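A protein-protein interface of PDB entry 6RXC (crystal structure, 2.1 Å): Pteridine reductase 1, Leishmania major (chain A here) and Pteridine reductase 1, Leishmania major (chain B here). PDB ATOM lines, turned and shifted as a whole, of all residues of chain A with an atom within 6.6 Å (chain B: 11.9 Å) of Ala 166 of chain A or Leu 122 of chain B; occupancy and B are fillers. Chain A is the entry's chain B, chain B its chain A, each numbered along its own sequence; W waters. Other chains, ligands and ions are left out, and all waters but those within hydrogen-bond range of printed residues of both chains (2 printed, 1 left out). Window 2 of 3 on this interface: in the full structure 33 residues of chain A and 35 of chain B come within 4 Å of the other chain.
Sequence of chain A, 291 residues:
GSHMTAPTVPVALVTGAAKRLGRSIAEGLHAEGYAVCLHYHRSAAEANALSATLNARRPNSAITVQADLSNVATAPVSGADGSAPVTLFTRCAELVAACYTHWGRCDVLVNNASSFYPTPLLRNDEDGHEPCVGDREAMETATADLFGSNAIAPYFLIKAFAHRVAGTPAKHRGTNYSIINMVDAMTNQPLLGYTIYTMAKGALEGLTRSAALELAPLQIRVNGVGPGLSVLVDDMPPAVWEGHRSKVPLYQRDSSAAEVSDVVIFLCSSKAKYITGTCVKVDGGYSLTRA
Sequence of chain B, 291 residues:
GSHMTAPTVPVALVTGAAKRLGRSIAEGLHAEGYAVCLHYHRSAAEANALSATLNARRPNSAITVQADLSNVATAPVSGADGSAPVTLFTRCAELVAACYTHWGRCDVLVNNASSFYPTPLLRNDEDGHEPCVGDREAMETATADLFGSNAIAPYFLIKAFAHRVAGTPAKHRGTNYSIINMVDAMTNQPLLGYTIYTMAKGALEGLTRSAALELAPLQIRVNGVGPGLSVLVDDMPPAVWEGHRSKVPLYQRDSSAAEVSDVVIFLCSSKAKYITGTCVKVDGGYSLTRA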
ATOM      1  N   LYS A 159       1.371  -8.038  15.707  1.00  0.00           N
ATOM      2  CA  LYS A 159       2.333  -6.965  15.735  1.00  0.00           C
ATOM      3  C   LYS A 159       2.986  -6.968  17.115  1.00  0.00           C
ATOM      4  O   LYS A 159       4.209  -6.945  17.221  1.00  0.00           O
ATOM      5  CB  LYS A 159       1.655  -5.621  15.434  1.00  0.00           C
ATOM      6  CG  LYS A 159       2.627  -4.453  15.381  1.00  0.00           C
ATOM      7  CD  LYS A 159       2.012  -3.087  15.159  1.00  0.00           C
ATOM      8  CE  LYS A 159       0.890  -3.060  14.134  1.00  0.00           C
ATOM      9  NZ  LYS A 159       0.949  -1.815  13.323  1.00  0.00           N
ATOM     10  N   PHE A 161       3.222  -9.402  19.077  1.00  0.00           N
ATOM     11  CA  PHE A 161       3.896 -10.668  19.355  1.00  0.00           C
ATOM     12  C   PHE A 161       5.288 -10.681  18.731  1.00  0.00           C
ATOM     13  O   PHE A 161       6.259 -11.148  19.321  1.00  0.00           O
ATOM     14  CB  PHE A 161       3.022 -11.804  18.833  1.00  0.00           C
ATOM     15  CG  PHE A 161       3.574 -13.204  18.960  1.00  0.00           C
ATOM     16  CD1 PHE A 161       4.551 -13.668  18.087  1.00  0.00           C
ATOM     17  CD2 PHE A 161       3.017 -14.091  19.865  1.00  0.00           C
ATOM     18  CE1 PHE A 161       5.037 -14.960  18.172  1.00  0.00           C
ATOM     19  CE2 PHE A 161       3.494 -15.394  19.952  1.00  0.00           C
ATOM     20  CZ  PHE A 161       4.503 -15.825  19.109  1.00  0.00           C
ATOM     21  N   ALA A 162       5.353 -10.091  17.546  1.00  0.00           N
ATOM     22  CA  ALA A 162       6.530 -10.072  16.693  1.00  0.00           C
ATOM     23  C   ALA A 162       7.572  -9.108  17.246  1.00  0.00           C
ATOM     24  O   ALA A 162       8.782  -9.386  17.178  1.00  0.00           O
ATOM     25  CB  ALA A 162       6.114  -9.680  15.285  1.00  0.00           C
ATOM     26  N   HIS A 163       7.070  -7.956  17.709  1.00  0.00           N
ATOM     27  CA  HIS A 163       7.895  -6.967  18.367  1.00  0.00           C
ATOM     28  C   HIS A 163       8.521  -7.604  19.592  1.00  0.00           C
ATOM     29  O   HIS A 163       9.631  -7.237  19.907  1.00  0.00           O
ATOM     30  CB  HIS A 163       7.086  -5.736  18.834  1.00  0.00           C
ATOM     31  CG  HIS A 163       6.652  -4.793  17.755  1.00  0.00           C
ATOM     32  ND1 HIS A 163       6.322  -3.462  18.025  1.00  0.00           N
ATOM     33  CD2 HIS A 163       6.461  -4.953  16.425  1.00  0.00           C
ATOM     34  CE1 HIS A 163       5.950  -2.859  16.902  1.00  0.00           C
ATOM     35  NE2 HIS A 163       6.030  -3.744  15.920  1.00  0.00           N
ATOM     36  N   ARG A 164       7.770  -8.440  20.315  1.00  0.00           N
ATOM     37  CA  ARG A 164       8.286  -9.072  21.561  1.00  0.00           C
ATOM     38  C   ARG A 164       9.493  -9.954  21.227  1.00  0.00           C
ATOM     39  O   ARG A 164      10.542  -9.805  21.885  1.00  0.00           O
ATOM     40  CB  ARG A 164       7.183  -9.887  22.243  1.00  0.00           C
ATOM     41  CG  ARG A 164       6.236  -9.058  23.100  1.00  0.00           C
ATOM     42  CD  ARG A 164       6.871  -7.765  23.577  1.00  0.00           C
ATOM     43  NE  ARG A 164       7.486  -7.901  24.890  1.00  0.00           N
ATOM     44  CZ  ARG A 164       6.829  -7.814  26.041  1.00  0.00           C
ATOM     45  NH1 ARG A 164       5.526  -7.590  26.045  1.00  0.00           N
ATOM     46  NH2 ARG A 164       7.477  -7.951  27.184  1.00  0.00           N
ATOM     47  N   VAL A 165       9.326 -10.832  20.238  1.00  0.00           N
ATOM     48  CA  VAL A 165      10.360 -11.753  19.792  1.00  0.00           C
ATOM     49  C   VAL A 165      11.540 -10.930  19.280  1.00  0.00           C
ATOM     50  O   VAL A 165      12.682 -11.188  19.651  1.00  0.00           O
ATOM     51  CB  VAL A 165       9.834 -12.704  18.713  1.00  0.00           C
ATOM     52  CG1 VAL A 165      10.862 -13.765  18.313  1.00  0.00           C
ATOM     53  CG2 VAL A 165       8.511 -13.334  19.125  1.00  0.00           C
ATOM     54  N   ALA A 166      11.244  -9.929  18.439  1.00  0.00           N
ATOM     55  CA  ALA A 166      12.272  -9.064  17.887  1.00  0.00           C
ATOM     56  C   ALA A 166      13.114  -8.484  19.022  1.00  0.00           C
ATOM     57  O   ALA A 166      14.309  -8.344  18.861  1.00  0.00           O
ATOM     58  CB  ALA A 166      11.658  -7.974  17.048  1.00  0.00           C
ATOM     59  N   GLY A 167      12.478  -8.176  20.160  1.00  0.00           N
ATOM     60  CA  GLY A 167      13.127  -7.492  21.268  1.00  0.00           C
ATOM     61  C   GLY A 167      13.600  -8.438  22.378  1.00  0.00           C
ATOM     62  O   GLY A 167      13.983  -7.983  23.464  1.00  0.00           O
ATOM     63  N   THR A 168      13.536  -9.744  22.094  1.00  0.00           N
ATOM     64  CA  THR A 168      14.268 -10.789  22.791  1.00  0.00           C
ATOM     65  C   THR A 168      15.581 -11.026  22.043  1.00  0.00           C
ATOM     66  O   THR A 168      15.572 -11.275  20.845  1.00  0.00           O
ATOM     67  CB  THR A 168      13.428 -12.069  22.934  1.00  0.00           C
ATOM     68  OG1 THR A 168      12.049 -11.747  22.772  1.00  0.00           O
ATOM     69  CG2 THR A 168      13.585 -12.744  24.275  1.00  0.00           C
ATOM     70  N   PRO A 169      16.761 -10.915  22.701  1.00  0.00           N
ATOM     71  CA  PRO A 169      18.032 -11.284  22.072  1.00  0.00           C
ATOM     72  C   PRO A 169      17.915 -12.692  21.508  1.00  0.00           C
ATOM     73  O   PRO A 169      17.184 -13.519  22.052  1.00  0.00           O
ATOM     74  CB  PRO A 169      19.027 -11.235  23.236  1.00  0.00           C
ATOM     75  CG  PRO A 169      18.143 -11.278  24.468  1.00  0.00           C
ATOM     76  CD  PRO A 169      16.939 -10.451  24.081  1.00  0.00           C
ATOM     77  N   ALA A 170      18.572 -12.915  20.363  1.00  0.00           N
ATOM     78  CA  ALA A 170      18.399 -14.168  19.640  1.00  0.00           C
ATOM     79  C   ALA A 170      18.619 -15.353  20.577  1.00  0.00           C
ATOM     80  O   ALA A 170      17.824 -16.292  20.566  1.00  0.00           O
ATOM     81  CB  ALA A 170      19.306 -14.235  18.439  1.00  0.00           C
ATOM     82  N   ARG A 173      15.643 -16.280  22.518  1.00  0.00           N
ATOM     83  CA  ARG A 173      14.407 -16.611  21.817  1.00  0.00           C
ATOM     84  C   ARG A 173      14.078 -18.099  21.998  1.00  0.00           C
ATOM     85  O   ARG A 173      14.948 -18.953  22.087  1.00  0.00           O
ATOM     86  CB  ARG A 173      14.499 -16.322  20.310  1.00  0.00           C
ATOM     87  CG  ARG A 173      14.793 -14.874  19.919  1.00  0.00           C
ATOM     88  CD  ARG A 173      14.868 -14.677  18.418  1.00  0.00           C
ATOM     89  NE  ARG A 173      14.848 -13.247  18.290  1.00  0.00           N
ATOM     90  CZ  ARG A 173      15.539 -12.584  17.390  1.00  0.00           C
ATOM     91  NH1 ARG A 173      16.271 -13.249  16.500  1.00  0.00           N
ATOM     92  NH2 ARG A 173      15.484 -11.259  17.386  1.00  0.00           N
ATOM     93  N   GLU A 214       6.389 -11.789   6.232  1.00  0.00           N
ATOM     94  CA  GLU A 214       7.131 -10.752   6.926  1.00  0.00           C
ATOM     95  C   GLU A 214       7.888 -11.322   8.133  1.00  0.00           C
ATOM     96  O   GLU A 214       8.928 -10.772   8.516  1.00  0.00           O
ATOM     97  CB  GLU A 214       6.151  -9.664   7.361  1.00  0.00           C
ATOM     98  CG  GLU A 214       6.837  -8.412   7.893  1.00  0.00           C
ATOM     99  CD  GLU A 214       6.117  -7.098   7.608  1.00  0.00           C
ATOM    100  OE1 GLU A 214       5.074  -7.085   6.822  1.00  0.00           O
ATOM    101  OE2 GLU A 214       6.608  -6.081   8.133  1.00  0.00           O
ATOM    102  N   LEU A 215       7.333 -12.356   8.778  1.00  0.00           N
ATOM    103  CA  LEU A 215       7.888 -12.729  10.075  1.00  0.00           C
ATOM    104  C   LEU A 215       8.820 -13.935   9.917  1.00  0.00           C
ATOM    105  O   LEU A 215       9.464 -14.381  10.867  1.00  0.00           O
ATOM    106  CB  LEU A 215       6.744 -12.992  11.069  1.00  0.00           C
ATOM    107  CG  LEU A 215       5.798 -11.815  11.299  1.00  0.00           C
ATOM    108  CD1 LEU A 215       4.729 -12.161  12.273  1.00  0.00           C
ATOM    109  CD2 LEU A 215       6.510 -10.520  11.696  1.00  0.00           C
ATOM    110  N   LEU A 218      12.106 -14.006  11.484  1.00  0.00           N
ATOM    111  CA  LEU A 218      12.123 -14.204  12.917  1.00  0.00           C
ATOM    112  C   LEU A 218      11.869 -15.672  13.225  1.00  0.00           C
ATOM    113  O   LEU A 218      11.834 -16.038  14.384  1.00  0.00           O
ATOM    114  CB  LEU A 218      11.098 -13.277  13.587  1.00  0.00           C
ATOM    115  CG  LEU A 218      11.551 -11.817  13.718  1.00  0.00           C
ATOM    116  CD1 LEU A 218      10.485 -10.931  14.364  1.00  0.00           C
ATOM    117  CD2 LEU A 218      12.858 -11.743  14.516  1.00  0.00           C
ATOM    118  N   ILE A 220       9.020 -16.892  12.982  1.00  0.00           N
ATOM    119  CA  ILE A 220       7.636 -16.986  13.418  1.00  0.00           C
ATOM    120  C   ILE A 220       6.806 -17.559  12.264  1.00  0.00           C
ATOM    121  O   ILE A 220       6.750 -16.977  11.182  1.00  0.00           O
ATOM    122  CB  ILE A 220       7.088 -15.627  13.911  1.00  0.00           C
ATOM    123  CG1 ILE A 220       7.890 -15.059  15.088  1.00  0.00           C
ATOM    124  CG2 ILE A 220       5.640 -15.741  14.295  1.00  0.00           C
ATOM    125  CD1 ILE A 220       7.494 -13.675  15.464  1.00  0.00           C
ATOM    126  N   PRO B 118       2.927   1.343   3.060  1.00  0.00           N
ATOM    127  CA  PRO B 118       3.382   0.231   3.882  1.00  0.00           C
ATOM    128  C   PRO B 118       2.826   0.306   5.300  1.00  0.00           C
ATOM    129  O   PRO B 118       2.630   1.402   5.812  1.00  0.00           O
ATOM    130  CB  PRO B 118       4.912   0.366   3.908  1.00  0.00           C
ATOM    131  CG  PRO B 118       5.284   1.504   2.988  1.00  0.00           C
ATOM    132  CD  PRO B 118       4.021   2.295   2.777  1.00  0.00           C
ATOM    133  N   THR B 119       2.546  -0.842   5.918  1.00  0.00           N
ATOM    134  CA  THR B 119       2.295  -0.873   7.354  1.00  0.00           C
ATOM    135  C   THR B 119       3.044  -2.079   7.935  1.00  0.00           C
ATOM    136  O   THR B 119       2.408  -3.065   8.336  1.00  0.00           O
ATOM    137  CB  THR B 119       0.815  -1.018   7.698  1.00  0.00           C
ATOM    138  OG1 THR B 119       0.472  -2.187   6.965  1.00  0.00           O
ATOM    139  CG2 THR B 119      -0.029   0.168   7.256  1.00  0.00           C
ATOM    140  N   PRO B 120       4.394  -1.973   8.044  1.00  0.00           N
ATOM    141  CA  PRO B 120       5.249  -3.093   8.410  1.00  0.00           C
ATOM    142  C   PRO B 120       4.946  -3.558   9.832  1.00  0.00           C
ATOM    143  O   PRO B 120       4.627  -2.766  10.711  1.00  0.00           O
ATOM    144  CB  PRO B 120       6.703  -2.595   8.217  1.00  0.00           C
ATOM    145  CG  PRO B 120       6.636  -1.082   7.975  1.00  0.00           C
ATOM    146  CD  PRO B 120       5.164  -0.732   7.811  1.00  0.00           C
ATOM    147  N   LEU B 121       4.989  -4.872  10.042  1.00  0.00           N
ATOM    148  CA  LEU B 121       4.683  -5.468  11.323  1.00  0.00           C
ATOM    149  C   LEU B 121       5.836  -5.202  12.284  1.00  0.00           C
ATOM    150  O   LEU B 121       5.637  -5.223  13.496  1.00  0.00           O
ATOM    151  CB  LEU B 121       4.555  -6.961  11.074  1.00  0.00           C
ATOM    152  CG  LEU B 121       3.178  -7.388  10.601  1.00  0.00           C
ATOM    153  CD1 LEU B 121       3.206  -8.887  10.338  1.00  0.00           C
ATOM    154  CD2 LEU B 121       2.175  -7.080  11.683  1.00  0.00           C
ATOM    155  N   LEU B 122       7.027  -4.929  11.721  1.00  0.00           N
ATOM    156  CA  LEU B 122       8.210  -4.774  12.537  1.00  0.00           C
ATOM    157  C   LEU B 122       8.854  -3.407  12.306  1.00  0.00           C
ATOM    158  O   LEU B 122       9.514  -3.180  11.293  1.00  0.00           O
ATOM    159  CB  LEU B 122       9.152  -5.932  12.225  1.00  0.00           C
ATOM    160  CG  LEU B 122       8.929  -7.183  13.061  1.00  0.00           C
ATOM    161  CD1 LEU B 122       9.182  -8.423  12.224  1.00  0.00           C
ATOM    162  CD2 LEU B 122       9.877  -7.155  14.261  1.00  0.00           C
ATOM    163  N   ARG B 123       8.634  -2.524  13.290  1.00  0.00           N
ATOM    164  CA  ARG B 123       9.211  -1.197  13.438  1.00  0.00           C
ATOM    165  C   ARG B 123       9.785  -1.093  14.862  1.00  0.00           C
ATOM    166  O   ARG B 123      10.598  -1.931  15.264  1.00  0.00           O
ATOM    167  CB  ARG B 123       8.137  -0.185  13.011  1.00  0.00           C
ATOM    168  CG  ARG B 123       8.329   1.264  13.443  1.00  0.00           C
ATOM    169  CD  ARG B 123       7.595   2.097  12.423  1.00  0.00           C
ATOM    170  NE  ARG B 123       8.040   1.601  11.134  1.00  0.00           N
ATOM    171  CZ  ARG B 123       7.549   1.957   9.958  1.00  0.00           C
ATOM    172  NH1 ARG B 123       6.560   2.831   9.879  1.00  0.00           N
ATOM    173  NH2 ARG B 123       8.050   1.428   8.853  1.00  0.00           N
ATOM    174  N   ASN B 124       9.339  -0.084  15.630  1.00  0.00           N
ATOM    175  CA  ASN B 124       9.824   0.233  16.970  1.00  0.00           C
ATOM    176  C   ASN B 124      11.285  -0.212  17.157  1.00  0.00           C
ATOM    177  O   ASN B 124      12.007   0.479  17.908  1.00  0.00           O
ATOM    178  CB  ASN B 124       8.874  -0.265  18.063  1.00  0.00           C
ATOM    179  N   MET B 139      -1.517   5.489  13.213  1.00  0.00           N
ATOM    180  CA  MET B 139      -1.797   4.069  13.119  1.00  0.00           C
ATOM    181  C   MET B 139      -3.307   3.915  12.974  1.00  0.00           C
ATOM    182  O   MET B 139      -3.793   3.010  12.292  1.00  0.00           O
ATOM    183  CB  MET B 139      -1.309   3.325  14.372  1.00  0.00           C
ATOM    184  CG  MET B 139      -1.785   1.856  14.471  1.00  0.00           C
ATOM    185  SD  MET B 139      -0.539   0.612  13.952  1.00  0.00           S
ATOM    186  CE  MET B 139      -0.841   0.479  12.185  1.00  0.00           C
ATOM    187  N   LEU B 191       3.065  -8.243  -0.960  1.00  0.00           N
ATOM    188  CA  LEU B 191       4.154  -7.304  -1.016  1.00  0.00           C
ATOM    189  C   LEU B 191       4.642  -7.108   0.416  1.00  0.00           C
ATOM    190  O   LEU B 191       3.831  -6.962   1.307  1.00  0.00           O
ATOM    191  CB  LEU B 191       3.541  -6.043  -1.650  1.00  0.00           C
ATOM    192  CG  LEU B 191       4.534  -4.988  -2.155  1.00  0.00           C
ATOM    193  CD1 LEU B 191       5.535  -5.570  -3.166  1.00  0.00           C
ATOM    194  CD2 LEU B 191       3.787  -3.783  -2.734  1.00  0.00           C
ATOM    195  N   LEU B 192       5.956  -7.140   0.644  1.00  0.00           N
ATOM    196  CA  LEU B 192       6.546  -7.077   1.977  1.00  0.00           C
ATOM    197  C   LEU B 192       6.240  -5.702   2.599  1.00  0.00           C
ATOM    198  O   LEU B 192       6.490  -4.669   1.983  1.00  0.00           O
ATOM    199  CB  LEU B 192       8.056  -7.266   1.741  1.00  0.00           C
ATOM    200  CG  LEU B 192       8.894  -8.066   2.760  1.00  0.00           C
ATOM    201  CD1 LEU B 192       8.075  -8.926   3.708  1.00  0.00           C
ATOM    202  CD2 LEU B 192       9.922  -8.932   2.055  1.00  0.00           C
ATOM    203  N   GLY B 193       5.650  -5.693   3.799  1.00  0.00           N
ATOM    204  CA  GLY B 193       5.399  -4.492   4.598  1.00  0.00           C
ATOM    205  C   GLY B 193       3.993  -3.889   4.439  1.00  0.00           C
ATOM    206  O   GLY B 193       3.646  -2.915   5.131  1.00  0.00           O
ATOM    207  N   TYR B 194       3.161  -4.493   3.565  1.00  0.00           N
ATOM    208  CA  TYR B 194       1.914  -3.852   3.168  1.00  0.00           C
ATOM    209  C   TYR B 194       0.689  -4.619   3.678  1.00  0.00           C
ATOM    210  O   TYR B 194      -0.249  -4.772   2.904  1.00  0.00           O
ATOM    211  CB  TYR B 194       1.844  -3.809   1.633  1.00  0.00           C
ATOM    212  CG  TYR B 194       2.609  -2.672   1.012  1.00  0.00           C
ATOM    213  CD1 TYR B 194       3.989  -2.739   0.816  1.00  0.00           C
ATOM    214  CD2 TYR B 194       1.935  -1.550   0.575  1.00  0.00           C
ATOM    215  CE1 TYR B 194       4.692  -1.673   0.261  1.00  0.00           C
ATOM    216  CE2 TYR B 194       2.602  -0.476   0.024  1.00  0.00           C
ATOM    217  CZ  TYR B 194       3.983  -0.520  -0.100  1.00  0.00           C
ATOM    218  OH  TYR B 194       4.580   0.557  -0.692  1.00  0.00           O
ATOM    219  N   THR B 195       0.699  -5.042   4.965  1.00  0.00           N
ATOM    220  CA  THR B 195      -0.190  -6.040   5.546  1.00  0.00           C
ATOM    221  C   THR B 195      -1.621  -5.524   5.570  1.00  0.00           C
ATOM    222  O   THR B 195      -2.544  -6.302   5.263  1.00  0.00           O
ATOM    223  CB  THR B 195       0.233  -6.448   6.973  1.00  0.00           C
ATOM    224  OG1 THR B 195       1.443  -7.191   6.916  1.00  0.00           O
ATOM    225  CG2 THR B 195      -0.749  -7.349   7.713  1.00  0.00           C
ATOM    226  N   ILE B 196      -1.823  -4.265   6.018  1.00  0.00           N
ATOM    227  CA  ILE B 196      -3.198  -3.779   6.097  1.00  0.00           C
ATOM    228  C   ILE B 196      -3.792  -3.692   4.708  1.00  0.00           C
ATOM    229  O   ILE B 196      -4.962  -3.949   4.489  1.00  0.00           O
ATOM    230  CB  ILE B 196      -3.343  -2.403   6.816  1.00  0.00           C
ATOM    231  CG1 ILE B 196      -2.782  -2.506   8.227  1.00  0.00           C
ATOM    232  CG2 ILE B 196      -4.822  -2.074   6.975  1.00  0.00           C
ATOM    233  CD1 ILE B 196      -3.734  -3.320   9.093  1.00  0.00           C
HETATM  234  O   HOH W   1       4.671  -2.789  13.904  1.00  0.00           O
HETATM  235  O   HOH W   2       3.838  -8.341   4.872  1.00  0.00           O
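The backbone carbonyl oxygen (O) of Leu 121 of chain B is in hydrogen-bond range of a ring nitrogen (NE2) of His 163 of chain A (2.9 Å).
The side-chain carboxylate (OE2) of Glu 214 of chain A sits at hydrogen-bond distance from the backbone NH (N) of Leu 121 of chain B, 2.8 Å away.
The side-chain amino group (NZ) of Lys 159 of chain A is in hydrogen-bond range of the side-chain sulfur (SD) of Met 139 of chain B (2.9 Å).
OE1 of Glu 214 of chain A lies within hydrogen-bond range of N of Gly 193 of chain B (3.4 Å).
The backbone NH (N) of Thr 119 of chain B sits at hydrogen-bond distance from the backbone carbonyl oxygen (O) of Gly 193 of chain B (2.5 Å).
The backbone NH of Thr 195 of chain B sits at hydrogen-bond distance from the side-chain hydroxyl of Thr 119 of chain B, 3.5 Å away.
The guanidinium group (NH2) of Arg 173 of chain A sits at hydrogen-bond distance from the backbone carbonyl oxygen (O) of Ala 166 of chain A (3.5 Å).
N of Ile 220 of chain A sits at hydrogen-bond distance from O of Leu 215 of chain A.
Among the printed residues, pairs that only touch across the chains: Glu 214 of chain A with Pro 120 of chain B (3.3 Å), Ala 166 of chain A with Leu 122 of chain B (3.4 Å), Leu 215 of chain A with Leu 122 of chain B (3.4 Å), Leu 218 of chain A with Leu 122 of chain B (3.5 Å), Glu 214 of chain A with Thr 195 of chain B (3.6 Å), Lys 159 of chain A with Leu 121 of chain B (3.6 Å), Glu 214 of chain A with Leu 122 of chain B (3.8 Å), Glu 214 of chain A with Leu 192 of chain B (3.8 Å), Ala 162 of chain A with Leu 122 of chain B (3.8 Å), His 163 of chain A with Arg 123 of chain B (3.9 Å) and Leu 215 of chain A with Leu 121 of chain B (3.9 Å).
Of the printed residues of chain B, Lys 159 of chain A touches Leu 121 (3.6 Å) and Met 139 (2.9 Å).
Of chain B, only Leu 122 comes within 4 Å of Ala 162 of chain A.
His 163 of chain A touches just these residues of chain B: Leu 121 and Arg 123.
No residue of chain B comes within 4 Å of Val 165 of chain A.
Ala 166 of chain A touches just one residue of chain B: Leu 122 (3.4 Å).
No residue of chain B comes within 4 Å of Gly 167 of chain A.
No residue of chain B comes within 4 Å of Thr 168 of chain A.
Printed residues of chain B within 4 Å of Glu 214 of chain A: Pro 120 (3.3 Å), Leu 121 (2.8 Å), Leu 122 (3.8 Å), Leu 192 (3.8 Å), Gly 193 (3.4 Å) and Thr 195 (3.6 Å).
Of chain B, only Leu 121 (3.9 Å) and Leu 122 (3.4 Å) come within 4 Å of Leu 215 of chain A.
Of chain A, only Ala 162, Ala 166, Glu 214, Leu 215 and Leu 218 come within 4 Å of Leu 122 of chain B.
Of the printed residues of chain A, Arg 123 of chain B touches His 163.
Of the printed residues of chain A, Met 139 of chain B touches Lys 159 (2.9 Å).
Leu 191 of chain B touches none of the printed residues of chain A.
Of the printed residues of chain A, Gly 193 of chain B touches Glu 214 (3.4 Å).
Printed residues of chain A within 4 Å of Thr 195 of chain B: Glu 214 (3.6 Å).
The nearest residue of chain A that does not touch Leu 122 of chain B is His 163 of chain A (4.2 Å).
Of the 16 printed residues of chain A, 7 touch a printed residue of chain B.
Of the 14 printed residues of chain B, 8 touch a printed residue of chain A.
Among the printed residues, 15 pairs touch across the chains.
Among the printed residues, no Asp or Glu carboxylate lies within 4 Å of a Lys or Arg side-chain nitrogen of the other chain.
Water W1 lies within hydrogen-bond range of a ring nitrogen (NE2) of His 163 of chain A, the backbone carbonyl oxygen (O) of Leu 121 of chain B and the backbone carbonyl oxygen (O) of Pro 120 of chain B.
Water W2 lies within hydrogen-bond range of the side-chain carboxylate (OE1) of Glu 214 of chain A, the side-chain hydroxyl (OG1) of Thr 195 of chain B and the backbone NH (N) of Gly 193 of chain B.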
